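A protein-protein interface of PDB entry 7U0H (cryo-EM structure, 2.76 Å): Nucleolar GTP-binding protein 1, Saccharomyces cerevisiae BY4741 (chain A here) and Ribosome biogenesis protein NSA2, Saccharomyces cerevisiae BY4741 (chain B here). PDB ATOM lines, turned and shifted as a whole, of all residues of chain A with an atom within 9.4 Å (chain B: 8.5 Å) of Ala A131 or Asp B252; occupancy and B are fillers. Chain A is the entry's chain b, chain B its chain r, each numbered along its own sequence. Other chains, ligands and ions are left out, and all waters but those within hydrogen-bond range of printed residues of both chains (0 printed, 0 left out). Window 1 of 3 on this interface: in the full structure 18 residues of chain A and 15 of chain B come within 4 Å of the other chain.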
ATOM      1  N   TYR A  46      -0.087  11.435 -13.129  1.00  0.00           N
ATOM      2  CA  TYR A  46       0.998  12.265 -12.612  1.00  0.00           C
ATOM      3  C   TYR A  46       1.970  11.485 -11.721  1.00  0.00           C
ATOM      4  O   TYR A  46       3.173  11.787 -11.713  1.00  0.00           O
ATOM      5  CB  TYR A  46       0.408  13.480 -11.902  1.00  0.00           C
ATOM      6  CG  TYR A  46      -0.186  14.468 -12.883  1.00  0.00           C
ATOM      7  CD1 TYR A  46       0.630  15.217 -13.717  1.00  0.00           C
ATOM      8  CD2 TYR A  46      -1.557  14.641 -12.985  1.00  0.00           C
ATOM      9  CE1 TYR A  46       0.101  16.111 -14.612  1.00  0.00           C
ATOM     10  CE2 TYR A  46      -2.098  15.534 -13.881  1.00  0.00           C
ATOM     11  CZ  TYR A  46      -1.265  16.268 -14.693  1.00  0.00           C
ATOM     12  OH  TYR A  46      -1.798  17.165 -15.588  1.00  0.00           O
ATOM     13  N   VAL A  50       6.062  11.236 -12.192  1.00  0.00           N
ATOM     14  CA  VAL A  50       7.081  11.456 -11.164  1.00  0.00           C
ATOM     15  C   VAL A  50       8.000  10.246 -11.058  1.00  0.00           C
ATOM     16  O   VAL A  50       9.235  10.370 -11.043  1.00  0.00           O
ATOM     17  CB  VAL A  50       6.416  11.773  -9.811  1.00  0.00           C
ATOM     18  CG1 VAL A  50       7.441  11.718  -8.682  1.00  0.00           C
ATOM     19  CG2 VAL A  50       5.731  13.130  -9.846  1.00  0.00           C
ATOM     20  N   VAL A 108      12.981  12.207  -3.036  1.00  0.00           N
ATOM     21  CA  VAL A 108      11.971  13.160  -3.496  1.00  0.00           C
ATOM     22  C   VAL A 108      10.910  12.458  -4.332  1.00  0.00           C
ATOM     23  O   VAL A 108       9.719  12.783  -4.251  1.00  0.00           O
ATOM     24  CB  VAL A 108      12.630  14.308  -4.280  1.00  0.00           C
ATOM     25  CG1 VAL A 108      11.581  15.129  -5.008  1.00  0.00           C
ATOM     26  CG2 VAL A 108      13.423  15.191  -3.349  1.00  0.00           C
ATOM     27  N   ALA A 109      11.323  11.505  -5.168  1.00  0.00           N
ATOM     28  CA  ALA A 109      10.352  10.770  -5.969  1.00  0.00           C
ATOM     29  C   ALA A 109       9.371  10.024  -5.075  1.00  0.00           C
ATOM     30  O   ALA A 109       8.147  10.126  -5.253  1.00  0.00           O
ATOM     31  CB  ALA A 109      11.069   9.805  -6.913  1.00  0.00           C
ATOM     32  N   TYR A 112       7.014  12.635  -3.212  1.00  0.00           N
ATOM     33  CA  TYR A 112       5.985  13.301  -3.993  1.00  0.00           C
ATOM     34  C   TYR A 112       4.961  12.320  -4.544  1.00  0.00           C
ATOM     35  O   TYR A 112       3.803  12.698  -4.721  1.00  0.00           O
ATOM     36  CB  TYR A 112       6.609  14.139  -5.107  1.00  0.00           C
ATOM     37  CG  TYR A 112       6.776  15.582  -4.693  1.00  0.00           C
ATOM     38  CD1 TYR A 112       5.759  16.502  -4.901  1.00  0.00           C
ATOM     39  CD2 TYR A 112       7.934  16.018  -4.066  1.00  0.00           C
ATOM     40  CE1 TYR A 112       5.898  17.818  -4.515  1.00  0.00           C
ATOM     41  CE2 TYR A 112       8.081  17.334  -3.676  1.00  0.00           C
ATOM     42  CZ  TYR A 112       7.060  18.230  -3.905  1.00  0.00           C
ATOM     43  OH  TYR A 112       7.197  19.540  -3.520  1.00  0.00           O
ATOM     44  N   LEU A 115       2.665  12.085  -1.640  1.00  0.00           N
ATOM     45  CA  LEU A 115       1.775  13.243  -1.579  1.00  0.00           C
ATOM     46  C   LEU A 115       0.705  13.187  -2.669  1.00  0.00           C
ATOM     47  O   LEU A 115      -0.458  13.524  -2.421  1.00  0.00           O
ATOM     48  CB  LEU A 115       2.579  14.538  -1.690  1.00  0.00           C
ATOM     49  CG  LEU A 115       3.618  14.825  -0.604  1.00  0.00           C
ATOM     50  CD1 LEU A 115       4.205  16.223  -0.756  1.00  0.00           C
ATOM     51  CD2 LEU A 115       3.020  14.635   0.779  1.00  0.00           C
ATOM     52  N   LEU A 116       1.085  12.772  -3.882  1.00  0.00           N
ATOM     53  CA  LEU A 116       0.139  12.631  -4.983  1.00  0.00           C
ATOM     54  C   LEU A 116      -0.933  11.595  -4.694  1.00  0.00           C
ATOM     55  O   LEU A 116      -1.997  11.639  -5.319  1.00  0.00           O
ATOM     56  CB  LEU A 116       0.876  12.248  -6.268  1.00  0.00           C
ATOM     57  CG  LEU A 116       1.419  13.345  -7.183  1.00  0.00           C
ATOM     58  CD1 LEU A 116       2.249  12.733  -8.294  1.00  0.00           C
ATOM     59  CD2 LEU A 116       0.286  14.162  -7.760  1.00  0.00           C
ATOM     60  N   PHE A 123      -5.502  20.254 -11.282  1.00  0.00           N
ATOM     61  CA  PHE A 123      -4.626  21.393 -11.029  1.00  0.00           C
ATOM     62  C   PHE A 123      -3.612  21.080  -9.937  1.00  0.00           C
ATOM     63  O   PHE A 123      -2.410  21.321 -10.100  1.00  0.00           O
ATOM     64  CB  PHE A 123      -5.453  22.620 -10.648  1.00  0.00           C
ATOM     65  CG  PHE A 123      -4.629  23.750 -10.112  1.00  0.00           C
ATOM     66  CD1 PHE A 123      -3.837  24.503 -10.960  1.00  0.00           C
ATOM     67  CD2 PHE A 123      -4.627  24.048  -8.762  1.00  0.00           C
ATOM     68  CE1 PHE A 123      -3.064  25.537 -10.473  1.00  0.00           C
ATOM     69  CE2 PHE A 123      -3.859  25.081  -8.270  1.00  0.00           C
ATOM     70  CZ  PHE A 123      -3.077  25.828  -9.128  1.00  0.00           C
ATOM     71  N   GLN A 124      -4.080  20.547  -8.807  1.00  0.00           N
ATOM     72  CA  GLN A 124      -3.169  20.262  -7.704  1.00  0.00           C
ATOM     73  C   GLN A 124      -2.202  19.140  -8.060  1.00  0.00           C
ATOM     74  O   GLN A 124      -1.019  19.195  -7.698  1.00  0.00           O
ATOM     75  CB  GLN A 124      -3.962  19.923  -6.441  1.00  0.00           C
ATOM     76  CG  GLN A 124      -3.123  19.903  -5.178  1.00  0.00           C
ATOM     77  CD  GLN A 124      -3.956  19.746  -3.922  1.00  0.00           C
ATOM     78  OE1 GLN A 124      -4.944  20.458  -3.724  1.00  0.00           O
ATOM     79  NE2 GLN A 124      -3.565  18.812  -3.067  1.00  0.00           N
ATOM     80  N   CYS A 125      -2.682  18.115  -8.771  1.00  0.00           N
ATOM     81  CA  CYS A 125      -1.794  17.039  -9.199  1.00  0.00           C
ATOM     82  C   CYS A 125      -0.709  17.556 -10.135  1.00  0.00           C
ATOM     83  O   CYS A 125       0.464  17.182 -10.008  1.00  0.00           O
ATOM     84  CB  CYS A 125      -2.602  15.928  -9.868  1.00  0.00           C
ATOM     85  SG  CYS A 125      -3.662  14.991  -8.747  1.00  0.00           S
ATOM     86  N   LYS A 126      -1.077  18.432 -11.072  1.00  0.00           N
ATOM     87  CA  LYS A 126      -0.090  19.036 -11.958  1.00  0.00           C
ATOM     88  C   LYS A 126       0.911  19.873 -11.175  1.00  0.00           C
ATOM     89  O   LYS A 126       2.112  19.853 -11.471  1.00  0.00           O
ATOM     90  CB  LYS A 126      -0.794  19.884 -13.014  1.00  0.00           C
ATOM     91  CG  LYS A 126       0.132  20.698 -13.888  1.00  0.00           C
ATOM     92  CD  LYS A 126      -0.659  21.539 -14.865  1.00  0.00           C
ATOM     93  CE  LYS A 126       0.245  22.243 -15.848  1.00  0.00           C
ATOM     94  NZ  LYS A 126      -0.539  22.835 -16.959  1.00  0.00           N
ATOM     95  N   GLN A 127       0.432  20.625 -10.181  1.00  0.00           N
ATOM     96  CA  GLN A 127       1.337  21.420  -9.355  1.00  0.00           C
ATOM     97  C   GLN A 127       2.346  20.538  -8.633  1.00  0.00           C
ATOM     98  O   GLN A 127       3.543  20.849  -8.602  1.00  0.00           O
ATOM     99  CB  GLN A 127       0.542  22.250  -8.350  1.00  0.00           C
ATOM    100  CG  GLN A 127      -0.192  23.406  -8.976  1.00  0.00           C
ATOM    101  CD  GLN A 127       0.729  24.271  -9.805  1.00  0.00           C
ATOM    102  OE1 GLN A 127       0.804  24.126 -11.025  1.00  0.00           O
ATOM    103  NE2 GLN A 127       1.442  25.173  -9.146  1.00  0.00           N
ATOM    104  N   LEU A 128       1.885  19.430  -8.055  1.00  0.00           N
ATOM    105  CA  LEU A 128       2.802  18.526  -7.366  1.00  0.00           C
ATOM    106  C   LEU A 128       3.804  17.907  -8.335  1.00  0.00           C
ATOM    107  O   LEU A 128       4.989  17.760  -8.009  1.00  0.00           O
ATOM    108  CB  LEU A 128       2.016  17.439  -6.632  1.00  0.00           C
ATOM    109  CG  LEU A 128       1.181  17.856  -5.418  1.00  0.00           C
ATOM    110  CD1 LEU A 128       0.339  16.695  -4.932  1.00  0.00           C
ATOM    111  CD2 LEU A 128       2.068  18.357  -4.299  1.00  0.00           C
ATOM    112  N   LYS A 129       3.343  17.526  -9.530  1.00  0.00           N
ATOM    113  CA  LYS A 129       4.242  16.962 -10.533  1.00  0.00           C
ATOM    114  C   LYS A 129       5.333  17.959 -10.906  1.00  0.00           C
ATOM    115  O   LYS A 129       6.521  17.612 -10.972  1.00  0.00           O
ATOM    116  CB  LYS A 129       3.433  16.548 -11.767  1.00  0.00           C
ATOM    117  CG  LYS A 129       4.143  15.614 -12.740  1.00  0.00           C
ATOM    118  CD  LYS A 129       4.976  16.357 -13.775  1.00  0.00           C
ATOM    119  CE  LYS A 129       4.116  17.023 -14.830  1.00  0.00           C
ATOM    120  NZ  LYS A 129       4.947  17.588 -15.931  1.00  0.00           N
ATOM    121  N   ARG A 130       4.939  19.209 -11.153  1.00  0.00           N
ATOM    122  CA  ARG A 130       5.913  20.242 -11.479  1.00  0.00           C
ATOM    123  C   ARG A 130       6.876  20.470 -10.325  1.00  0.00           C
ATOM    124  O   ARG A 130       8.070  20.685 -10.545  1.00  0.00           O
ATOM    125  CB  ARG A 130       5.206  21.544 -11.853  1.00  0.00           C
ATOM    126  CG  ARG A 130       4.892  21.674 -13.330  1.00  0.00           C
ATOM    127  CD  ARG A 130       4.610  23.121 -13.707  1.00  0.00           C
ATOM    128  NE  ARG A 130       5.753  23.987 -13.436  1.00  0.00           N
ATOM    129  CZ  ARG A 130       6.676  24.316 -14.330  1.00  0.00           C
ATOM    130  NH1 ARG A 130       6.624  23.871 -15.574  1.00  0.00           N
ATOM    131  NH2 ARG A 130       7.677  25.112 -13.966  1.00  0.00           N
ATOM    132  N   ALA A 131       6.378  20.425  -9.087  1.00  0.00           N
ATOM    133  CA  ALA A 131       7.251  20.614  -7.933  1.00  0.00           C
ATOM    134  C   ALA A 131       8.299  19.512  -7.844  1.00  0.00           C
ATOM    135  O   ALA A 131       9.482  19.786  -7.606  1.00  0.00           O
ATOM    136  CB  ALA A 131       6.420  20.673  -6.652  1.00  0.00           C
ATOM    137  N   ALA A 132       7.885  18.261  -8.042  1.00  0.00           N
ATOM    138  CA  ALA A 132       8.829  17.148  -7.992  1.00  0.00           C
ATOM    139  C   ALA A 132       9.890  17.275  -9.082  1.00  0.00           C
ATOM    140  O   ALA A 132      11.098  17.145  -8.816  1.00  0.00           O
ATOM    141  CB  ALA A 132       8.081  15.824  -8.117  1.00  0.00           C
ATOM    142  N   LEU A 133       9.459  17.544 -10.319  1.00  0.00           N
ATOM    143  CA  LEU A 133      10.424  17.662 -11.408  1.00  0.00           C
ATOM    144  C   LEU A 133      11.344  18.861 -11.201  1.00  0.00           C
ATOM    145  O   LEU A 133      12.535  18.797 -11.523  1.00  0.00           O
ATOM    146  CB  LEU A 133       9.712  17.761 -12.757  1.00  0.00           C
ATOM    147  CG  LEU A 133       8.704  16.690 -13.185  1.00  0.00           C
ATOM    148  CD1 LEU A 133       8.521  16.716 -14.703  1.00  0.00           C
ATOM    149  CD2 LEU A 133       9.092  15.299 -12.711  1.00  0.00           C
ATOM    150  N   GLY A 134      10.815  19.959 -10.658  1.00  0.00           N
ATOM    151  CA  GLY A 134      11.647  21.121 -10.395  1.00  0.00           C
ATOM    152  C   GLY A 134      12.689  20.874  -9.320  1.00  0.00           C
ATOM    153  O   GLY A 134      13.827  21.334  -9.433  1.00  0.00           O
ATOM    154  N   ARG A 135      12.316  20.155  -8.258  1.00  0.00           N
ATOM    155  CA  ARG A 135      13.297  19.786  -7.240  1.00  0.00           C
ATOM    156  C   ARG A 135      14.401  18.918  -7.829  1.00  0.00           C
ATOM    157  O   ARG A 135      15.591  19.130  -7.550  1.00  0.00           O
ATOM    158  CB  ARG A 135      12.613  19.059  -6.085  1.00  0.00           C
ATOM    159  CG  ARG A 135      11.854  19.951  -5.129  1.00  0.00           C
ATOM    160  CD  ARG A 135      11.073  19.104  -4.145  1.00  0.00           C
ATOM    161  NE  ARG A 135      10.455  19.894  -3.089  1.00  0.00           N
ATOM    162  CZ  ARG A 135      10.900  19.957  -1.841  1.00  0.00           C
ATOM    163  NH1 ARG A 135      11.965  19.277  -1.452  1.00  0.00           N
ATOM    164  NH2 ARG A 135      10.256  20.717  -0.962  1.00  0.00           N
ATOM    165  N   MET A 136      14.025  17.934  -8.652  1.00  0.00           N
ATOM    166  CA  MET A 136      15.041  17.099  -9.291  1.00  0.00           C
ATOM    167  C   MET A 136      15.947  17.928 -10.197  1.00  0.00           C
ATOM    168  O   MET A 136      17.165  17.715 -10.238  1.00  0.00           O
ATOM    169  CB  MET A 136      14.376  15.974 -10.079  1.00  0.00           C
ATOM    170  CG  MET A 136      13.508  15.048  -9.245  1.00  0.00           C
ATOM    171  SD  MET A 136      12.680  13.814 -10.266  1.00  0.00           S
ATOM    172  CE  MET A 136      11.765  12.890  -9.043  1.00  0.00           C
ATOM    173  N   ALA A 137      15.366  18.879 -10.933  1.00  0.00           N
ATOM    174  CA  ALA A 137      16.161  19.743 -11.800  1.00  0.00           C
ATOM    175  C   ALA A 137      17.131  20.594 -10.994  1.00  0.00           C
ATOM    176  O   ALA A 137      18.276  20.803 -11.409  1.00  0.00           O
ATOM    177  CB  ALA A 137      15.241  20.627 -12.635  1.00  0.00           C
ATOM    178  N   THR A 138      16.683  21.108  -9.848  1.00  0.00           N
ATOM    179  CA  THR A 138      17.570  21.870  -8.974  1.00  0.00           C
ATOM    180  C   THR A 138      18.735  21.014  -8.497  1.00  0.00           C
ATOM    181  O   THR A 138      19.885  21.470  -8.478  1.00  0.00           O
ATOM    182  CB  THR A 138      16.785  22.419  -7.781  1.00  0.00           C
ATOM    183  OG1 THR A 138      15.726  23.265  -8.247  1.00  0.00           O
ATOM    184  CG2 THR A 138      17.692  23.219  -6.862  1.00  0.00           C
ATOM    185  N   ILE A 139      18.457  19.767  -8.111  1.00  0.00           N
ATOM    186  CA  ILE A 139      19.530  18.868  -7.687  1.00  0.00           C
ATOM    187  C   ILE A 139      20.538  18.676  -8.814  1.00  0.00           C
ATOM    188  O   ILE A 139      21.755  18.805  -8.619  1.00  0.00           O
ATOM    189  CB  ILE A 139      18.954  17.521  -7.222  1.00  0.00           C
ATOM    190  CG1 ILE A 139      18.114  17.705  -5.961  1.00  0.00           C
ATOM    191  CG2 ILE A 139      20.068  16.518  -6.998  1.00  0.00           C
ATOM    192  CD1 ILE A 139      17.397  16.455  -5.536  1.00  0.00           C
ATOM    193  N   HIS B 154      -2.207  20.071   4.355  1.00  0.00           N
ATOM    194  CA  HIS B 154      -1.044  19.750   5.172  1.00  0.00           C
ATOM    195  C   HIS B 154      -1.245  20.177   6.622  1.00  0.00           C
ATOM    196  O   HIS B 154      -1.754  21.266   6.904  1.00  0.00           O
ATOM    197  CB  HIS B 154       0.204  20.421   4.592  1.00  0.00           C
ATOM    198  CG  HIS B 154       0.742  19.741   3.373  1.00  0.00           C
ATOM    199  ND1 HIS B 154       0.164  18.610   2.835  1.00  0.00           N
ATOM    200  CD2 HIS B 154       1.814  20.022   2.594  1.00  0.00           C
ATOM    201  CE1 HIS B 154       0.853  18.228   1.775  1.00  0.00           C
ATOM    202  NE2 HIS B 154       1.856  19.069   1.604  1.00  0.00           N
ATOM    203  N   GLN B 179       3.812  17.976   8.151  1.00  0.00           N
ATOM    204  CA  GLN B 179       5.045  18.716   7.933  1.00  0.00           C
ATOM    205  C   GLN B 179       5.661  19.051   9.282  1.00  0.00           C
ATOM    206  O   GLN B 179       4.989  19.617  10.150  1.00  0.00           O
ATOM    207  CB  GLN B 179       4.782  19.996   7.134  1.00  0.00           C
ATOM    208  CG  GLN B 179       4.317  19.759   5.711  1.00  0.00           C
ATOM    209  CD  GLN B 179       5.322  18.979   4.890  1.00  0.00           C
ATOM    210  OE1 GLN B 179       6.529  19.201   4.997  1.00  0.00           O
ATOM    211  NE2 GLN B 179       4.832  18.062   4.060  1.00  0.00           N
ATOM    212  N   THR B 246       3.905  31.677   3.745  1.00  0.00           N
ATOM    213  CA  THR B 246       3.579  32.566   2.640  1.00  0.00           C
ATOM    214  C   THR B 246       2.915  31.878   1.455  1.00  0.00           C
ATOM    215  O   THR B 246       2.250  32.555   0.662  1.00  0.00           O
ATOM    216  CB  THR B 246       4.849  33.278   2.159  1.00  0.00           C
ATOM    217  OG1 THR B 246       5.894  32.316   1.971  1.00  0.00           O
ATOM    218  CG2 THR B 246       5.299  34.301   3.182  1.00  0.00           C
ATOM    219  N   ASN B 247       3.064  30.564   1.313  1.00  0.00           N
ATOM    220  CA  ASN B 247       2.564  29.846   0.151  1.00  0.00           C
ATOM    221  C   ASN B 247       1.703  28.678   0.602  1.00  0.00           C
ATOM    222  O   ASN B 247       1.827  28.186   1.725  1.00  0.00           O
ATOM    223  CB  ASN B 247       3.710  29.330  -0.724  1.00  0.00           C
ATOM    224  CG  ASN B 247       4.603  28.349   0.014  1.00  0.00           C
ATOM    225  OD1 ASN B 247       4.747  28.424   1.230  1.00  0.00           O
ATOM    226  ND2 ASN B 247       5.202  27.422  -0.721  1.00  0.00           N
ATOM    227  N   GLU B 248       0.828  28.230  -0.290  1.00  0.00           N
ATOM    228  CA  GLU B 248       0.028  27.047  -0.008  1.00  0.00           C
ATOM    229  C   GLU B 248       0.918  25.813  -0.042  1.00  0.00           C
ATOM    230  O   GLU B 248       1.494  25.505  -1.093  1.00  0.00           O
ATOM    231  CB  GLU B 248      -1.108  26.905  -1.014  1.00  0.00           C
ATOM    232  CG  GLU B 248      -2.417  27.508  -0.559  1.00  0.00           C
ATOM    233  CD  GLU B 248      -2.972  26.833   0.679  1.00  0.00           C
ATOM    234  OE1 GLU B 248      -2.754  25.614   0.850  1.00  0.00           O
ATOM    235  OE2 GLU B 248      -3.622  27.524   1.487  1.00  0.00           O
ATOM    236  N   PRO B 249       1.054  25.078   1.065  1.00  0.00           N
ATOM    237  CA  PRO B 249       1.920  23.893   1.045  1.00  0.00           C
ATOM    238  C   PRO B 249       1.355  22.739   0.241  1.00  0.00           C
ATOM    239  O   PRO B 249       2.133  21.940  -0.292  1.00  0.00           O
ATOM    240  CB  PRO B 249       2.051  23.533   2.532  1.00  0.00           C
ATOM    241  CG  PRO B 249       0.819  24.063   3.149  1.00  0.00           C
ATOM    242  CD  PRO B 249       0.498  25.332   2.404  1.00  0.00           C
ATOM    243  N   ASP B 250       0.029  22.628   0.124  1.00  0.00           N
ATOM    244  CA  ASP B 250      -0.578  21.484  -0.546  1.00  0.00           C
ATOM    245  C   ASP B 250      -0.298  21.451  -2.044  1.00  0.00           C
ATOM    246  O   ASP B 250      -0.600  20.442  -2.688  1.00  0.00           O
ATOM    247  CB  ASP B 250      -2.087  21.461  -0.294  1.00  0.00           C
ATOM    248  CG  ASP B 250      -2.742  22.807  -0.521  1.00  0.00           C
ATOM    249  OD1 ASP B 250      -2.119  23.677  -1.162  1.00  0.00           O
ATOM    250  OD2 ASP B 250      -3.882  22.996  -0.053  1.00  0.00           O
ATOM    251  N   ARG B 251       0.248  22.526  -2.609  1.00  0.00           N
ATOM    252  CA  ARG B 251       0.698  22.541  -3.996  1.00  0.00           C
ATOM    253  C   ARG B 251       2.206  22.347  -4.091  1.00  0.00           C
ATOM    254  O   ARG B 251       2.680  21.415  -4.746  1.00  0.00           O
ATOM    255  CB  ARG B 251       0.299  23.860  -4.671  1.00  0.00           C
ATOM    256  CG  ARG B 251      -1.179  24.191  -4.606  1.00  0.00           C
ATOM    257  CD  ARG B 251      -1.428  25.610  -5.102  1.00  0.00           C
ATOM    258  NE  ARG B 251      -2.834  25.987  -5.010  1.00  0.00           N
ATOM    259  CZ  ARG B 251      -3.275  27.237  -5.027  1.00  0.00           C
ATOM    260  NH1 ARG B 251      -2.445  28.261  -5.136  1.00  0.00           N
ATOM    261  NH2 ARG B 251      -4.579  27.465  -4.914  1.00  0.00           N
ATOM    262  N   ASP B 252       2.971  23.211  -3.427  1.00  0.00           N
ATOM    263  CA  ASP B 252       4.422  23.195  -3.542  1.00  0.00           C
ATOM    264  C   ASP B 252       5.064  21.992  -2.867  1.00  0.00           C
ATOM    265  O   ASP B 252       6.254  21.749  -3.092  1.00  0.00           O
ATOM    266  CB  ASP B 252       5.004  24.481  -2.954  1.00  0.00           C
ATOM    267  CG  ASP B 252       4.596  25.713  -3.732  1.00  0.00           C
ATOM    268  OD1 ASP B 252       4.024  25.563  -4.830  1.00  0.00           O
ATOM    269  OD2 ASP B 252       4.849  26.836  -3.245  1.00  0.00           O
ATOM    270  N   GLY B 253       4.324  21.243  -2.053  1.00  0.00           N
ATOM    271  CA  GLY B 253       4.893  20.097  -1.378  1.00  0.00           C
ATOM    272  C   GLY B 253       5.808  20.423  -0.221  1.00  0.00           C
ATOM    273  O   GLY B 253       6.473  19.518   0.293  1.00  0.00           O
ATOM    274  N   CYS B 254       5.867  21.684   0.204  1.00  0.00           N
ATOM    275  CA  CYS B 254       6.751  22.109   1.281  1.00  0.00           C
ATOM    276  C   CYS B 254       6.151  23.338   1.950  1.00  0.00           C
ATOM    277  O   CYS B 254       5.109  23.849   1.536  1.00  0.00           O
ATOM    278  CB  CYS B 254       8.158  22.407   0.766  1.00  0.00           C
ATOM    279  SG  CYS B 254       8.240  23.769  -0.417  1.00  0.00           S
ATOM    280  N   VAL B 255       6.826  23.815   2.992  1.00  0.00           N
ATOM    281  CA  VAL B 255       6.364  24.949   3.783  1.00  0.00           C
ATOM    282  C   VAL B 255       7.427  26.038   3.738  1.00  0.00           C
ATOM    283  O   VAL B 255       8.590  25.798   4.088  1.00  0.00           O
ATOM    284  CB  VAL B 255       6.059  24.545   5.232  1.00  0.00           C
ATOM    285  CG1 VAL B 255       5.287  25.644   5.924  1.00  0.00           C
ATOM    286  CG2 VAL B 255       5.285  23.246   5.267  1.00  0.00           C
ATOM    287  N   ASN B 256       7.026  27.232   3.314  1.00  0.00           N
ATOM    288  CA  ASN B 256       7.900  28.393   3.281  1.00  0.00           C
ATOM    289  C   ASN B 256       7.280  29.499   4.116  1.00  0.00           C
ATOM    290  O   ASN B 256       6.106  29.835   3.931  1.00  0.00           O
ATOM    291  CB  ASN B 256       8.138  28.863   1.849  1.00  0.00           C
ATOM    292  CG  ASN B 256       8.940  27.867   1.042  1.00  0.00           C
ATOM    293  OD1 ASN B 256       9.864  27.238   1.556  1.00  0.00           O
ATOM    294  ND2 ASN B 256       8.584  27.708  -0.228  1.00  0.00           N
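The side-chain amide nitrogen (NE2) of Gln A124 is in hydrogen-bond range of the backbone carbonyl oxygen (O) of Asp B250, at 3.4 Å. OH of Tyr A112 sits at hydrogen-bond distance from O of Asp B252, at 2.4 Å. The guanidinium group of Arg A135 sits close to the side-chain sulfur of Cys B254, 3.7 Å away.
Of the 24 printed residues of chain A, 8 touch a printed residue of chain B. Among the printed residues, 10 pairs touch across the chains. Among the printed residues, no Asp or Glu carboxylate lies within 4 Å of a Lys or Arg side-chain nitrogen of the other chain.
Ala A131 touches just one residue of chain B: Asp B252 (3.7 Å). Of chain A, only Tyr A112 (2.4 Å) and Ala A131 (3.7 Å) come within 4 Å of Asp B252. Of the printed residues of chain B, Gln A127 touches Arg B251 (3.99 Å). Of the printed residues of chain B, Tyr A112 touches Asp B252 (2.4 Å) and Gly B253 (3.2 Å). Of the printed residues of chain A, Asp B250 touches Gln A124 (3.4 Å) and Leu A128 (3.7 Å). Lys A126 touches none of the printed residues of chain B. Ala A109 touches none of the printed residues of chain B. The nearest printed residue of chain B that does not touch Leu A128 is Gly B253 (4.3 Å).
The side-chain hydroxyl (OH) of Tyr A112 is in hydrogen-bond range of the guanidinium group (NE) of Arg A135 (3.3 Å). The side-chain amide nitrogen of Asn B247 sits at hydrogen-bond distance from the side-chain carboxylate of Asp B252 (2.6 Å).
Among the printed residues, merely in contact across the chains: Leu A128 with Arg B251 (3.2 Å), Tyr A112 with Gly B253 (3.2 Å), Phe A123 with Arg B251 (3.5 Å), Ala A131 with Asp B252 (3.7 Å), Leu A128 with Asp B250 (3.7 Å), Leu A115 with Gly B253 (3.98 Å) and Gln A127 with Arg B251 (3.99 Å).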
